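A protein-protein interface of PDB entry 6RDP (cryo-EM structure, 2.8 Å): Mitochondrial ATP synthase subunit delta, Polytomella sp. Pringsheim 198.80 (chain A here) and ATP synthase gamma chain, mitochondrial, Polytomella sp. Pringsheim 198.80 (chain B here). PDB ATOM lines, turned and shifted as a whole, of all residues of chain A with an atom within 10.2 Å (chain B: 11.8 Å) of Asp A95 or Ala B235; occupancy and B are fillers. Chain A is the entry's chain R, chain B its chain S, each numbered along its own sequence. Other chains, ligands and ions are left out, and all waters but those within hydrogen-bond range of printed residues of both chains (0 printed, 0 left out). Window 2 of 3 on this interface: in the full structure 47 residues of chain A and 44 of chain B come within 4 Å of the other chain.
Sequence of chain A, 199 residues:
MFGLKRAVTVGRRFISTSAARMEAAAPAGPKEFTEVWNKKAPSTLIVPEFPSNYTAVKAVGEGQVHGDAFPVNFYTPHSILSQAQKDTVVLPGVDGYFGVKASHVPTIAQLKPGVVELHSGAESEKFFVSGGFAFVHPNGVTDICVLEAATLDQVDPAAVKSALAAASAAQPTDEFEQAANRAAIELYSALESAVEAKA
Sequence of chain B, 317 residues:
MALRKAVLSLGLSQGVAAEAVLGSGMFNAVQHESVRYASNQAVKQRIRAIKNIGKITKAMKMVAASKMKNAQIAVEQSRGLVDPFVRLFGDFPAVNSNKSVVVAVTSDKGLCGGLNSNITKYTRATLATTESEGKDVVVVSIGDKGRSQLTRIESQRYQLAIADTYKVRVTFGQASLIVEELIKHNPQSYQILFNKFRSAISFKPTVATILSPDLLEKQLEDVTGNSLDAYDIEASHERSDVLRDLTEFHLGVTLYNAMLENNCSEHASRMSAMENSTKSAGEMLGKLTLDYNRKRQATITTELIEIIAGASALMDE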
ATOM      1  N   LEU A  91       2.737 -15.870 -10.780  1.00  0.00           N
ATOM      2  CA  LEU A  91       3.898 -16.457 -10.140  1.00  0.00           C
ATOM      3  C   LEU A  91       4.297 -15.649  -8.922  1.00  0.00           C
ATOM      4  O   LEU A  91       4.392 -14.421  -9.010  1.00  0.00           O
ATOM      5  CB  LEU A  91       5.057 -16.515 -11.121  1.00  0.00           C
ATOM      6  CG  LEU A  91       4.865 -17.535 -12.224  1.00  0.00           C
ATOM      7  CD1 LEU A  91       5.879 -17.348 -13.309  1.00  0.00           C
ATOM      8  CD2 LEU A  91       5.007 -18.886 -11.603  1.00  0.00           C
ATOM      9  N   PRO A  92       4.533 -16.276  -7.790  1.00  0.00           N
ATOM     10  CA  PRO A  92       4.902 -15.547  -6.564  1.00  0.00           C
ATOM     11  C   PRO A  92       6.400 -15.312  -6.370  1.00  0.00           C
ATOM     12  O   PRO A  92       7.057 -15.920  -5.531  1.00  0.00           O
ATOM     13  CB  PRO A  92       4.347 -16.453  -5.469  1.00  0.00           C
ATOM     14  CG  PRO A  92       4.456 -17.817  -6.042  1.00  0.00           C
ATOM     15  CD  PRO A  92       4.301 -17.702  -7.528  1.00  0.00           C
ATOM     16  N   GLY A  93       6.959 -14.384  -7.146  1.00  0.00           N
ATOM     17  CA  GLY A  93       8.376 -14.076  -7.081  1.00  0.00           C
ATOM     18  C   GLY A  93       8.783 -13.445  -5.759  1.00  0.00           C
ATOM     19  O   GLY A  93       7.964 -13.145  -4.893  1.00  0.00           O
ATOM     20  N   VAL A  94      10.092 -13.251  -5.598  1.00  0.00           N
ATOM     21  CA  VAL A  94      10.570 -12.747  -4.316  1.00  0.00           C
ATOM     22  C   VAL A  94      10.379 -11.243  -4.171  1.00  0.00           C
ATOM     23  O   VAL A  94      10.409 -10.732  -3.044  1.00  0.00           O
ATOM     24  CB  VAL A  94      12.042 -13.108  -4.070  1.00  0.00           C
ATOM     25  CG1 VAL A  94      12.193 -14.593  -3.934  1.00  0.00           C
ATOM     26  CG2 VAL A  94      12.902 -12.596  -5.180  1.00  0.00           C
ATOM     27  N   ASP A  95      10.179 -10.511  -5.266  1.00  0.00           N
ATOM     28  CA  ASP A  95       9.780  -9.120  -5.125  1.00  0.00           C
ATOM     29  C   ASP A  95       8.296  -9.007  -4.838  1.00  0.00           C
ATOM     30  O   ASP A  95       7.866  -8.070  -4.158  1.00  0.00           O
ATOM     31  CB  ASP A  95      10.122  -8.337  -6.391  1.00  0.00           C
ATOM     32  CG  ASP A  95      11.606  -8.285  -6.661  1.00  0.00           C
ATOM     33  OD1 ASP A  95      11.988  -7.891  -7.776  1.00  0.00           O
ATOM     34  OD2 ASP A  95      12.394  -8.646  -5.759  1.00  0.00           O
ATOM     35  N   GLY A  96       7.523  -9.957  -5.317  1.00  0.00           N
ATOM     36  CA  GLY A  96       6.088  -9.959  -5.142  1.00  0.00           C
ATOM     37  C   GLY A  96       5.458 -10.751  -6.265  1.00  0.00           C
ATOM     38  O   GLY A  96       6.134 -11.216  -7.175  1.00  0.00           O
ATOM     39  N   TYR A  97       4.139 -10.892  -6.176  1.00  0.00           N
ATOM     40  CA  TYR A  97       3.397 -11.645  -7.177  1.00  0.00           C
ATOM     41  C   TYR A  97       3.440 -10.927  -8.513  1.00  0.00           C
ATOM     42  O   TYR A  97       3.140  -9.736  -8.595  1.00  0.00           O
ATOM     43  CB  TYR A  97       1.947 -11.819  -6.742  1.00  0.00           C
ATOM     44  CG  TYR A  97       1.705 -12.907  -5.732  1.00  0.00           C
ATOM     45  CD1 TYR A  97       2.122 -12.768  -4.422  1.00  0.00           C
ATOM     46  CD2 TYR A  97       1.033 -14.062  -6.088  1.00  0.00           C
ATOM     47  CE1 TYR A  97       1.893 -13.755  -3.499  1.00  0.00           C
ATOM     48  CE2 TYR A  97       0.801 -15.053  -5.174  1.00  0.00           C
ATOM     49  CZ  TYR A  97       1.230 -14.893  -3.882  1.00  0.00           C
ATOM     50  OH  TYR A  97       1.000 -15.882  -2.959  1.00  0.00           O
ATOM     51  N   PHE A  98       3.820 -11.641  -9.558  1.00  0.00           N
ATOM     52  CA  PHE A  98       3.769 -11.096 -10.897  1.00  0.00           C
ATOM     53  C   PHE A  98       2.995 -12.050 -11.786  1.00  0.00           C
ATOM     54  O   PHE A  98       2.606 -13.142 -11.371  1.00  0.00           O
ATOM     55  CB  PHE A  98       5.168 -10.808 -11.457  1.00  0.00           C
ATOM     56  CG  PHE A  98       5.998 -12.023 -11.748  1.00  0.00           C
ATOM     57  CD1 PHE A  98       6.657 -12.696 -10.735  1.00  0.00           C
ATOM     58  CD2 PHE A  98       6.186 -12.445 -13.052  1.00  0.00           C
ATOM     59  CE1 PHE A  98       7.443 -13.789 -11.012  1.00  0.00           C
ATOM     60  CE2 PHE A  98       6.970 -13.538 -13.333  1.00  0.00           C
ATOM     61  CZ  PHE A  98       7.598 -14.209 -12.313  1.00  0.00           C
ATOM     62  N   THR A 107      12.722 -14.258 -18.366  1.00  0.00           N
ATOM     63  CA  THR A 107      12.774 -14.074 -16.924  1.00  0.00           C
ATOM     64  C   THR A 107      13.389 -15.319 -16.299  1.00  0.00           C
ATOM     65  O   THR A 107      13.152 -16.429 -16.772  1.00  0.00           O
ATOM     66  CB  THR A 107      11.361 -13.841 -16.354  1.00  0.00           C
ATOM     67  OG1 THR A 107      10.696 -12.820 -17.103  1.00  0.00           O
ATOM     68  CG2 THR A 107      11.399 -13.402 -14.906  1.00  0.00           C
ATOM     69  N   ILE A 108      14.203 -15.129 -15.265  1.00  0.00           N
ATOM     70  CA  ILE A 108      14.586 -16.194 -14.342  1.00  0.00           C
ATOM     71  C   ILE A 108      14.177 -15.702 -12.963  1.00  0.00           C
ATOM     72  O   ILE A 108      14.901 -14.924 -12.336  1.00  0.00           O
ATOM     73  CB  ILE A 108      16.080 -16.520 -14.396  1.00  0.00           C
ATOM     74  CG1 ILE A 108      16.472 -17.015 -15.777  1.00  0.00           C
ATOM     75  CG2 ILE A 108      16.441 -17.584 -13.381  1.00  0.00           C
ATOM     76  CD1 ILE A 108      17.951 -17.021 -15.996  1.00  0.00           C
ATOM     77  N   ALA A 109      13.019 -16.123 -12.490  1.00  0.00           N
ATOM     78  CA  ALA A 109      12.443 -15.560 -11.280  1.00  0.00           C
ATOM     79  C   ALA A 109      12.507 -16.575 -10.157  1.00  0.00           C
ATOM     80  O   ALA A 109      11.950 -17.667 -10.273  1.00  0.00           O
ATOM     81  CB  ALA A 109      11.001 -15.130 -11.520  1.00  0.00           C
ATOM     82  N   GLN A 110      13.185 -16.220  -9.078  1.00  0.00           N
ATOM     83  CA  GLN A 110      13.131 -17.023  -7.871  1.00  0.00           C
ATOM     84  C   GLN A 110      11.809 -16.761  -7.177  1.00  0.00           C
ATOM     85  O   GLN A 110      11.421 -15.608  -6.998  1.00  0.00           O
ATOM     86  CB  GLN A 110      14.290 -16.692  -6.939  1.00  0.00           C
ATOM     87  CG  GLN A 110      14.301 -17.527  -5.677  1.00  0.00           C
ATOM     88  CD  GLN A 110      15.472 -17.210  -4.780  1.00  0.00           C
ATOM     89  OE1 GLN A 110      16.388 -16.489  -5.166  1.00  0.00           O
ATOM     90  NE2 GLN A 110      15.451 -17.753  -3.571  1.00  0.00           N
ATOM     91  N   LEU A 111      11.109 -17.820  -6.805  1.00  0.00           N
ATOM     92  CA  LEU A 111       9.802 -17.683  -6.189  1.00  0.00           C
ATOM     93  C   LEU A 111       9.896 -17.866  -4.685  1.00  0.00           C
ATOM     94  O   LEU A 111      10.543 -18.794  -4.197  1.00  0.00           O
ATOM     95  CB  LEU A 111       8.809 -18.685  -6.761  1.00  0.00           C
ATOM     96  CG  LEU A 111       8.651 -18.730  -8.279  1.00  0.00           C
ATOM     97  CD1 LEU A 111       7.598 -19.748  -8.621  1.00  0.00           C
ATOM     98  CD2 LEU A 111       8.313 -17.389  -8.862  1.00  0.00           C
ATOM     99  N   LYS A 112       9.259 -16.965  -3.958  1.00  0.00           N
ATOM    100  CA  LYS A 112       9.012 -17.150  -2.543  1.00  0.00           C
ATOM    101  C   LYS A 112       7.823 -18.085  -2.401  1.00  0.00           C
ATOM    102  O   LYS A 112       7.103 -18.319  -3.373  1.00  0.00           O
ATOM    103  CB  LYS A 112       8.771 -15.788  -1.886  1.00  0.00           C
ATOM    104  CG  LYS A 112       7.423 -15.158  -2.189  1.00  0.00           C
ATOM    105  CD  LYS A 112       7.373 -13.715  -1.711  1.00  0.00           C
ATOM    106  CE  LYS A 112       7.440 -13.620  -0.194  1.00  0.00           C
ATOM    107  NZ  LYS A 112       7.324 -12.209   0.284  1.00  0.00           N
ATOM    108  N   PRO A 113       7.620 -18.688  -1.217  1.00  0.00           N
ATOM    109  CA  PRO A 113       6.430 -19.524  -1.015  1.00  0.00           C
ATOM    110  C   PRO A 113       5.118 -18.787  -1.200  1.00  0.00           C
ATOM    111  O   PRO A 113       4.758 -17.931  -0.393  1.00  0.00           O
ATOM    112  CB  PRO A 113       6.592 -19.996   0.428  1.00  0.00           C
ATOM    113  CG  PRO A 113       8.038 -20.057   0.617  1.00  0.00           C
ATOM    114  CD  PRO A 113       8.610 -18.912  -0.148  1.00  0.00           C
ATOM    115  N   PHE A 133      12.514 -21.917  -8.489  1.00  0.00           N
ATOM    116  CA  PHE A 133      12.594 -20.944  -9.562  1.00  0.00           C
ATOM    117  C   PHE A 133      11.511 -21.169 -10.607  1.00  0.00           C
ATOM    118  O   PHE A 133      10.873 -22.215 -10.672  1.00  0.00           O
ATOM    119  CB  PHE A 133      13.976 -20.999 -10.198  1.00  0.00           C
ATOM    120  CG  PHE A 133      15.079 -20.805  -9.217  1.00  0.00           C
ATOM    121  CD1 PHE A 133      15.525 -19.538  -8.922  1.00  0.00           C
ATOM    122  CD2 PHE A 133      15.651 -21.881  -8.565  1.00  0.00           C
ATOM    123  CE1 PHE A 133      16.515 -19.347  -8.009  1.00  0.00           C
ATOM    124  CE2 PHE A 133      16.638 -21.689  -7.662  1.00  0.00           C
ATOM    125  CZ  PHE A 133      17.074 -20.419  -7.382  1.00  0.00           C
ATOM    126  N   ALA A 134      11.308 -20.149 -11.433  1.00  0.00           N
ATOM    127  CA  ALA A 134      10.340 -20.204 -12.518  1.00  0.00           C
ATOM    128  C   ALA A 134      10.887 -19.381 -13.668  1.00  0.00           C
ATOM    129  O   ALA A 134      11.059 -18.172 -13.528  1.00  0.00           O
ATOM    130  CB  ALA A 134       8.987 -19.665 -12.080  1.00  0.00           C
ATOM    131  N   GLU A 186       8.260 -17.195   7.537  1.00  0.00           N
ATOM    132  CA  GLU A 186       7.863 -16.545   6.297  1.00  0.00           C
ATOM    133  C   GLU A 186       6.973 -17.442   5.449  1.00  0.00           C
ATOM    134  O   GLU A 186       5.957 -16.972   4.923  1.00  0.00           O
ATOM    135  CB  GLU A 186       9.114 -16.119   5.536  1.00  0.00           C
ATOM    136  CG  GLU A 186       8.857 -15.202   4.372  1.00  0.00           C
ATOM    137  CD  GLU A 186      10.141 -14.657   3.792  1.00  0.00           C
ATOM    138  OE1 GLU A 186      11.226 -15.077   4.246  1.00  0.00           O
ATOM    139  OE2 GLU A 186      10.067 -13.785   2.905  1.00  0.00           O
ATOM    140  N   LEU B 228      22.477 -15.711 -21.749  1.00  0.00           N
ATOM    141  CA  LEU B 228      21.863 -15.629 -20.432  1.00  0.00           C
ATOM    142  C   LEU B 228      21.326 -14.239 -20.134  1.00  0.00           C
ATOM    143  O   LEU B 228      20.450 -14.092 -19.276  1.00  0.00           O
ATOM    144  CB  LEU B 228      22.878 -16.026 -19.360  1.00  0.00           C
ATOM    145  CG  LEU B 228      22.388 -16.419 -17.974  1.00  0.00           C
ATOM    146  CD1 LEU B 228      21.689 -17.758 -18.024  1.00  0.00           C
ATOM    147  CD2 LEU B 228      23.556 -16.448 -17.020  1.00  0.00           C
ATOM    148  N   TYR B 231      17.374 -12.848 -20.080  1.00  0.00           N
ATOM    149  CA  TYR B 231      16.440 -13.047 -18.983  1.00  0.00           C
ATOM    150  C   TYR B 231      16.589 -11.960 -17.934  1.00  0.00           C
ATOM    151  O   TYR B 231      17.703 -11.563 -17.588  1.00  0.00           O
ATOM    152  CB  TYR B 231      16.661 -14.410 -18.327  1.00  0.00           C
ATOM    153  CG  TYR B 231      16.754 -15.570 -19.287  1.00  0.00           C
ATOM    154  CD1 TYR B 231      15.615 -16.200 -19.756  1.00  0.00           C
ATOM    155  CD2 TYR B 231      17.986 -16.043 -19.714  1.00  0.00           C
ATOM    156  CE1 TYR B 231      15.697 -17.256 -20.639  1.00  0.00           C
ATOM    157  CE2 TYR B 231      18.077 -17.095 -20.594  1.00  0.00           C
ATOM    158  CZ  TYR B 231      16.931 -17.695 -21.051  1.00  0.00           C
ATOM    159  OH  TYR B 231      17.027 -18.747 -21.922  1.00  0.00           O
ATOM    160  N   ASP B 232      15.459 -11.495 -17.416  1.00  0.00           N
ATOM    161  CA  ASP B 232      15.469 -10.565 -16.295  1.00  0.00           C
ATOM    162  C   ASP B 232      15.590 -11.342 -14.997  1.00  0.00           C
ATOM    163  O   ASP B 232      14.660 -12.050 -14.606  1.00  0.00           O
ATOM    164  CB  ASP B 232      14.204  -9.713 -16.270  1.00  0.00           C
ATOM    165  CG  ASP B 232      14.026  -8.907 -17.524  1.00  0.00           C
ATOM    166  OD1 ASP B 232      12.865  -8.612 -17.867  1.00  0.00           O
ATOM    167  OD2 ASP B 232      15.045  -8.574 -18.164  1.00  0.00           O
ATOM    168  N   ILE B 233      16.725 -11.195 -14.323  1.00  0.00           N
ATOM    169  CA  ILE B 233      16.925 -11.857 -13.043  1.00  0.00           C
ATOM    170  C   ILE B 233      16.037 -11.201 -11.998  1.00  0.00           C
ATOM    171  O   ILE B 233      16.200 -10.021 -11.675  1.00  0.00           O
ATOM    172  CB  ILE B 233      18.394 -11.799 -12.624  1.00  0.00           C
ATOM    173  CG1 ILE B 233      19.273 -12.406 -13.714  1.00  0.00           C
ATOM    174  CG2 ILE B 233      18.573 -12.484 -11.299  1.00  0.00           C
ATOM    175  CD1 ILE B 233      18.944 -13.832 -14.018  1.00  0.00           C
ATOM    176  N   GLU B 234      15.108 -11.969 -11.453  1.00  0.00           N
ATOM    177  CA  GLU B 234      14.153 -11.476 -10.477  1.00  0.00           C
ATOM    178  C   GLU B 234      14.484 -12.074  -9.117  1.00  0.00           C
ATOM    179  O   GLU B 234      13.620 -12.506  -8.369  1.00  0.00           O
ATOM    180  CB  GLU B 234      12.731 -11.795 -10.939  1.00  0.00           C
ATOM    181  CG  GLU B 234      11.580 -10.959 -10.357  1.00  0.00           C
ATOM    182  CD  GLU B 234      10.874 -11.618  -9.187  1.00  0.00           C
ATOM    183  OE1 GLU B 234      10.872 -12.853  -9.108  1.00  0.00           O
ATOM    184  OE2 GLU B 234      10.307 -10.899  -8.343  1.00  0.00           O
ATOM    185  N   ALA B 235      15.764 -12.133  -8.790  1.00  0.00           N
ATOM    186  CA  ALA B 235      16.201 -12.689  -7.524  1.00  0.00           C
ATOM    187  C   ALA B 235      16.147 -11.623  -6.439  1.00  0.00           C
ATOM    188  O   ALA B 235      15.762 -10.478  -6.674  1.00  0.00           O
ATOM    189  CB  ALA B 235      17.610 -13.265  -7.650  1.00  0.00           C
ATOM    190  N   SER B 236      16.521 -12.017  -5.225  1.00  0.00           N
ATOM    191  CA  SER B 236      16.743 -11.033  -4.175  1.00  0.00           C
ATOM    192  C   SER B 236      18.098 -10.364  -4.348  1.00  0.00           C
ATOM    193  O   SER B 236      18.205  -9.134  -4.330  1.00  0.00           O
ATOM    194  CB  SER B 236      16.647 -11.691  -2.802  1.00  0.00           C
ATOM    195  OG  SER B 236      17.847 -12.370  -2.494  1.00  0.00           O
ATOM    196  N   HIS B 237      19.146 -11.165  -4.508  1.00  0.00           N
ATOM    197  CA  HIS B 237      20.509 -10.718  -4.702  1.00  0.00           C
ATOM    198  C   HIS B 237      20.905 -10.873  -6.170  1.00  0.00           C
ATOM    199  O   HIS B 237      20.046 -11.057  -7.038  1.00  0.00           O
ATOM    200  CB  HIS B 237      21.416 -11.467  -3.739  1.00  0.00           C
ATOM    201  CG  HIS B 237      21.200 -11.087  -2.310  1.00  0.00           C
ATOM    202  ND1 HIS B 237      20.051 -11.408  -1.621  1.00  0.00           N
ATOM    203  CD2 HIS B 237      21.975 -10.394  -1.445  1.00  0.00           C
ATOM    204  CE1 HIS B 237      20.133 -10.938  -0.389  1.00  0.00           C
ATOM    205  NE2 HIS B 237      21.291 -10.321  -0.255  1.00  0.00           N
ATOM    206  N   GLU B 238      22.200 -10.760  -6.447  1.00  0.00           N
ATOM    207  CA  GLU B 238      22.701 -10.625  -7.807  1.00  0.00           C
ATOM    208  C   GLU B 238      22.579 -11.935  -8.583  1.00  0.00           C
ATOM    209  O   GLU B 238      22.222 -12.984  -8.045  1.00  0.00           O
ATOM    210  CB  GLU B 238      24.151 -10.159  -7.781  1.00  0.00           C
ATOM    211  CG  GLU B 238      24.319  -8.670  -7.566  1.00  0.00           C
ATOM    212  CD  GLU B 238      24.083  -7.880  -8.831  1.00  0.00           C
ATOM    213  OE1 GLU B 238      23.325  -6.888  -8.787  1.00  0.00           O
ATOM    214  OE2 GLU B 238      24.652  -8.256  -9.874  1.00  0.00           O
ATOM    215  N   ARG B 239      22.906 -11.855  -9.877  1.00  0.00           N
ATOM    216  CA  ARG B 239      22.842 -13.008 -10.772  1.00  0.00           C
ATOM    217  C   ARG B 239      23.844 -14.088 -10.390  1.00  0.00           C
ATOM    218  O   ARG B 239      23.561 -15.282 -10.546  1.00  0.00           O
ATOM    219  CB  ARG B 239      23.079 -12.555 -12.212  1.00  0.00           C
ATOM    220  CG  ARG B 239      22.959 -13.661 -13.236  1.00  0.00           C
ATOM    221  CD  ARG B 239      22.835 -13.157 -14.642  1.00  0.00           C
ATOM    222  NE  ARG B 239      24.053 -12.507 -15.094  1.00  0.00           N
ATOM    223  CZ  ARG B 239      24.295 -12.209 -16.362  1.00  0.00           C
ATOM    224  NH1 ARG B 239      23.400 -12.514 -17.288  1.00  0.00           N
ATOM    225  NH2 ARG B 239      25.427 -11.611 -16.703  1.00  0.00           N
ATOM    226  N   SER B 240      24.989 -13.695  -9.838  1.00  0.00           N
ATOM    227  CA  SER B 240      26.008 -14.634  -9.390  1.00  0.00           C
ATOM    228  C   SER B 240      25.548 -15.521  -8.245  1.00  0.00           C
ATOM    229  O   SER B 240      26.183 -16.546  -7.984  1.00  0.00           O
ATOM    230  CB  SER B 240      27.252 -13.860  -8.956  1.00  0.00           C
ATOM    231  OG  SER B 240      28.227 -14.732  -8.420  1.00  0.00           O
ATOM    232  N   ASP B 241      24.473 -15.156  -7.556  1.00  0.00           N
ATOM    233  CA  ASP B 241      23.894 -15.971  -6.509  1.00  0.00           C
ATOM    234  C   ASP B 241      22.639 -16.702  -6.959  1.00  0.00           C
ATOM    235  O   ASP B 241      22.359 -17.793  -6.448  1.00  0.00           O
ATOM    236  CB  ASP B 241      23.591 -15.093  -5.299  1.00  0.00           C
ATOM    237  CG  ASP B 241      24.820 -14.358  -4.815  1.00  0.00           C
ATOM    238  OD1 ASP B 241      25.929 -14.691  -5.277  1.00  0.00           O
ATOM    239  OD2 ASP B 241      24.684 -13.412  -4.018  1.00  0.00           O
ATOM    240  N   VAL B 242      21.902 -16.162  -7.927  1.00  0.00           N
ATOM    241  CA  VAL B 242      20.791 -16.920  -8.472  1.00  0.00           C
ATOM    242  C   VAL B 242      21.305 -18.078  -9.322  1.00  0.00           C
ATOM    243  O   VAL B 242      20.699 -19.147  -9.319  1.00  0.00           O
ATOM    244  CB  VAL B 242      19.801 -16.021  -9.245  1.00  0.00           C
ATOM    245  CG1 VAL B 242      20.252 -15.703 -10.643  1.00  0.00           C
ATOM    246  CG2 VAL B 242      18.450 -16.649  -9.298  1.00  0.00           C
ATOM    247  N   LEU B 243      22.473 -17.946  -9.960  1.00  0.00           N
ATOM    248  CA  LEU B 243      23.043 -19.105 -10.637  1.00  0.00           C
ATOM    249  C   LEU B 243      23.686 -20.061  -9.654  1.00  0.00           C
ATOM    250  O   LEU B 243      23.717 -21.266  -9.907  1.00  0.00           O
ATOM    251  CB  LEU B 243      24.051 -18.685 -11.698  1.00  0.00           C
ATOM    252  CG  LEU B 243      23.512 -18.508 -13.111  1.00  0.00           C
ATOM    253  CD1 LEU B 243      22.603 -17.316 -13.251  1.00  0.00           C
ATOM    254  CD2 LEU B 243      24.671 -18.398 -14.063  1.00  0.00           C
ATOM    255  N   ARG B 244      24.168 -19.540  -8.529  1.00  0.00           N
ATOM    256  CA  ARG B 244      24.698 -20.389  -7.473  1.00  0.00           C
ATOM    257  C   ARG B 244      23.613 -21.278  -6.892  1.00  0.00           C
ATOM    258  O   ARG B 244      23.832 -22.472  -6.684  1.00  0.00           O
ATOM    259  CB  ARG B 244      25.332 -19.520  -6.389  1.00  0.00           C
ATOM    260  CG  ARG B 244      25.575 -20.197  -5.065  1.00  0.00           C
ATOM    261  CD  ARG B 244      26.675 -21.227  -5.150  1.00  0.00           C
ATOM    262  NE  ARG B 244      27.861 -20.719  -5.823  1.00  0.00           N
ATOM    263  CZ  ARG B 244      28.999 -21.398  -5.928  1.00  0.00           C
ATOM    264  NH1 ARG B 244      30.036 -20.868  -6.565  1.00  0.00           N
ATOM    265  NH2 ARG B 244      29.103 -22.608  -5.393  1.00  0.00           N
ATOM    266  N   ASP B 245      22.427 -20.725  -6.653  1.00  0.00           N
ATOM    267  CA  ASP B 245      21.308 -21.545  -6.199  1.00  0.00           C
ATOM    268  C   ASP B 245      20.768 -22.421  -7.321  1.00  0.00           C
ATOM    269  O   ASP B 245      20.364 -23.569  -7.089  1.00  0.00           O
ATOM    270  CB  ASP B 245      20.199 -20.653  -5.650  1.00  0.00           C
ATOM    271  CG  ASP B 245      20.665 -19.775  -4.506  1.00  0.00           C
ATOM    272  OD1 ASP B 245      21.655 -20.137  -3.838  1.00  0.00           O
ATOM    273  OD2 ASP B 245      20.036 -18.722  -4.271  1.00  0.00           O
ATOM    274  N   LEU B 246      20.797 -21.911  -8.548  1.00  0.00           N
ATOM    275  CA  LEU B 246      20.163 -22.588  -9.664  1.00  0.00           C
ATOM    276  C   LEU B 246      20.953 -23.811 -10.106  1.00  0.00           C
ATOM    277  O   LEU B 246      20.360 -24.811 -10.513  1.00  0.00           O
ATOM    278  CB  LEU B 246      19.991 -21.576 -10.795  1.00  0.00           C
ATOM    279  CG  LEU B 246      19.042 -21.823 -11.948  1.00  0.00           C
ATOM    280  CD1 LEU B 246      17.729 -22.211 -11.399  1.00  0.00           C
ATOM    281  CD2 LEU B 246      18.887 -20.555 -12.737  1.00  0.00           C
ATOM    282  N   THR B 247      22.278 -23.788  -9.969  1.00  0.00           N
ATOM    283  CA  THR B 247      23.054 -24.969 -10.327  1.00  0.00           C
ATOM    284  C   THR B 247      23.044 -26.026  -9.235  1.00  0.00           C
ATOM    285  O   THR B 247      23.171 -27.209  -9.545  1.00  0.00           O
ATOM    286  CB  THR B 247      24.493 -24.603 -10.659  1.00  0.00           C
ATOM    287  OG1 THR B 247      25.044 -23.832  -9.591  1.00  0.00           O
ATOM    288  CG2 THR B 247      24.539 -23.817 -11.942  1.00  0.00           C
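The backbone NH (N) of Asp A95 lies within hydrogen-bond range of the side-chain carboxylate (OE2) of Glu B234, 3.1 Å away. N of Ile A108 is in hydrogen-bond range of O of Asp B232, at 3.2 Å. O of Ile A108 is in hydrogen-bond range of N of Glu B234 (3.1 Å).
The backbone NH of Val A94 lies within hydrogen-bond range of the backbone carbonyl oxygen of Gln A110, at 3.0 Å. O of Ala A109 sits at hydrogen-bond distance from N of Ala A134 (2.8 Å). A ring nitrogen (ND1) of His B237 is in hydrogen-bond range of the side-chain hydroxyl of Ser B236, at 2.6 Å.
Among the printed residues, pairs that only touch across the chains: Gly A93 with Glu B234 (3.4 Å), Val A94 with Glu B234 (3.3 Å), Val A94 with Ala B235 (3.6 Å), Val A94 with Ser B236 (3.7 Å), Asp A95 with Ala B235 (3.9 Å), Thr A107 with Tyr B231 (3.8 Å), Thr A107 with Asp B232 (3.5 Å), Ile A108 with Tyr B231 (3.7 Å), Ile A108 with Ile B233 (3.7 Å), Ile A108 with Leu B246 (3.9 Å), Ala A109 with Glu B234 (3.3 Å), Gln A110 with Glu B234 (3.5 Å), Phe A133 with Val B242 (3.6 Å), Phe A133 with Asp B245 (3.6 Å) and Phe A133 with Leu B246 (3.5 Å).
Ala B235 touches just these residues of chain A: Val A94 and Asp A95. Val A94 touches three residues of chain B. Of chain B, only Glu B234 comes within 4 Å of Ala A109. Of chain B, only Glu B234 comes within 4 Å of Gln A110. Printed residues of chain A within 4 Å of Glu B234: Gly A93, Val A94, Asp A95, Ile A108, Ala A109 and Gln A110. Ser B236 touches one residue of chain A. Printed residues of chain A within 4 Å of Asp B245: Phe A133 (3.6 Å). Of the printed residues of chain A, Asp B232 touches Thr A107 and Ile A108. The nearest residue of chain B that does not touch Asp A95 is Ser B236 (5.2 Å). The nearest printed residue of chain A that does not touch Tyr B231 is Ala A109 (7.1 Å).
Hydrophobic or aromatic side chains of chain B that line the printed part of chain A: Tyr B231, Ile B233, Val B242 and Leu B246. Hydrophobic or aromatic side chains of chain A that line the printed part of chain B: Val A94, Ile A108, Ala A109 and Phe A133.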
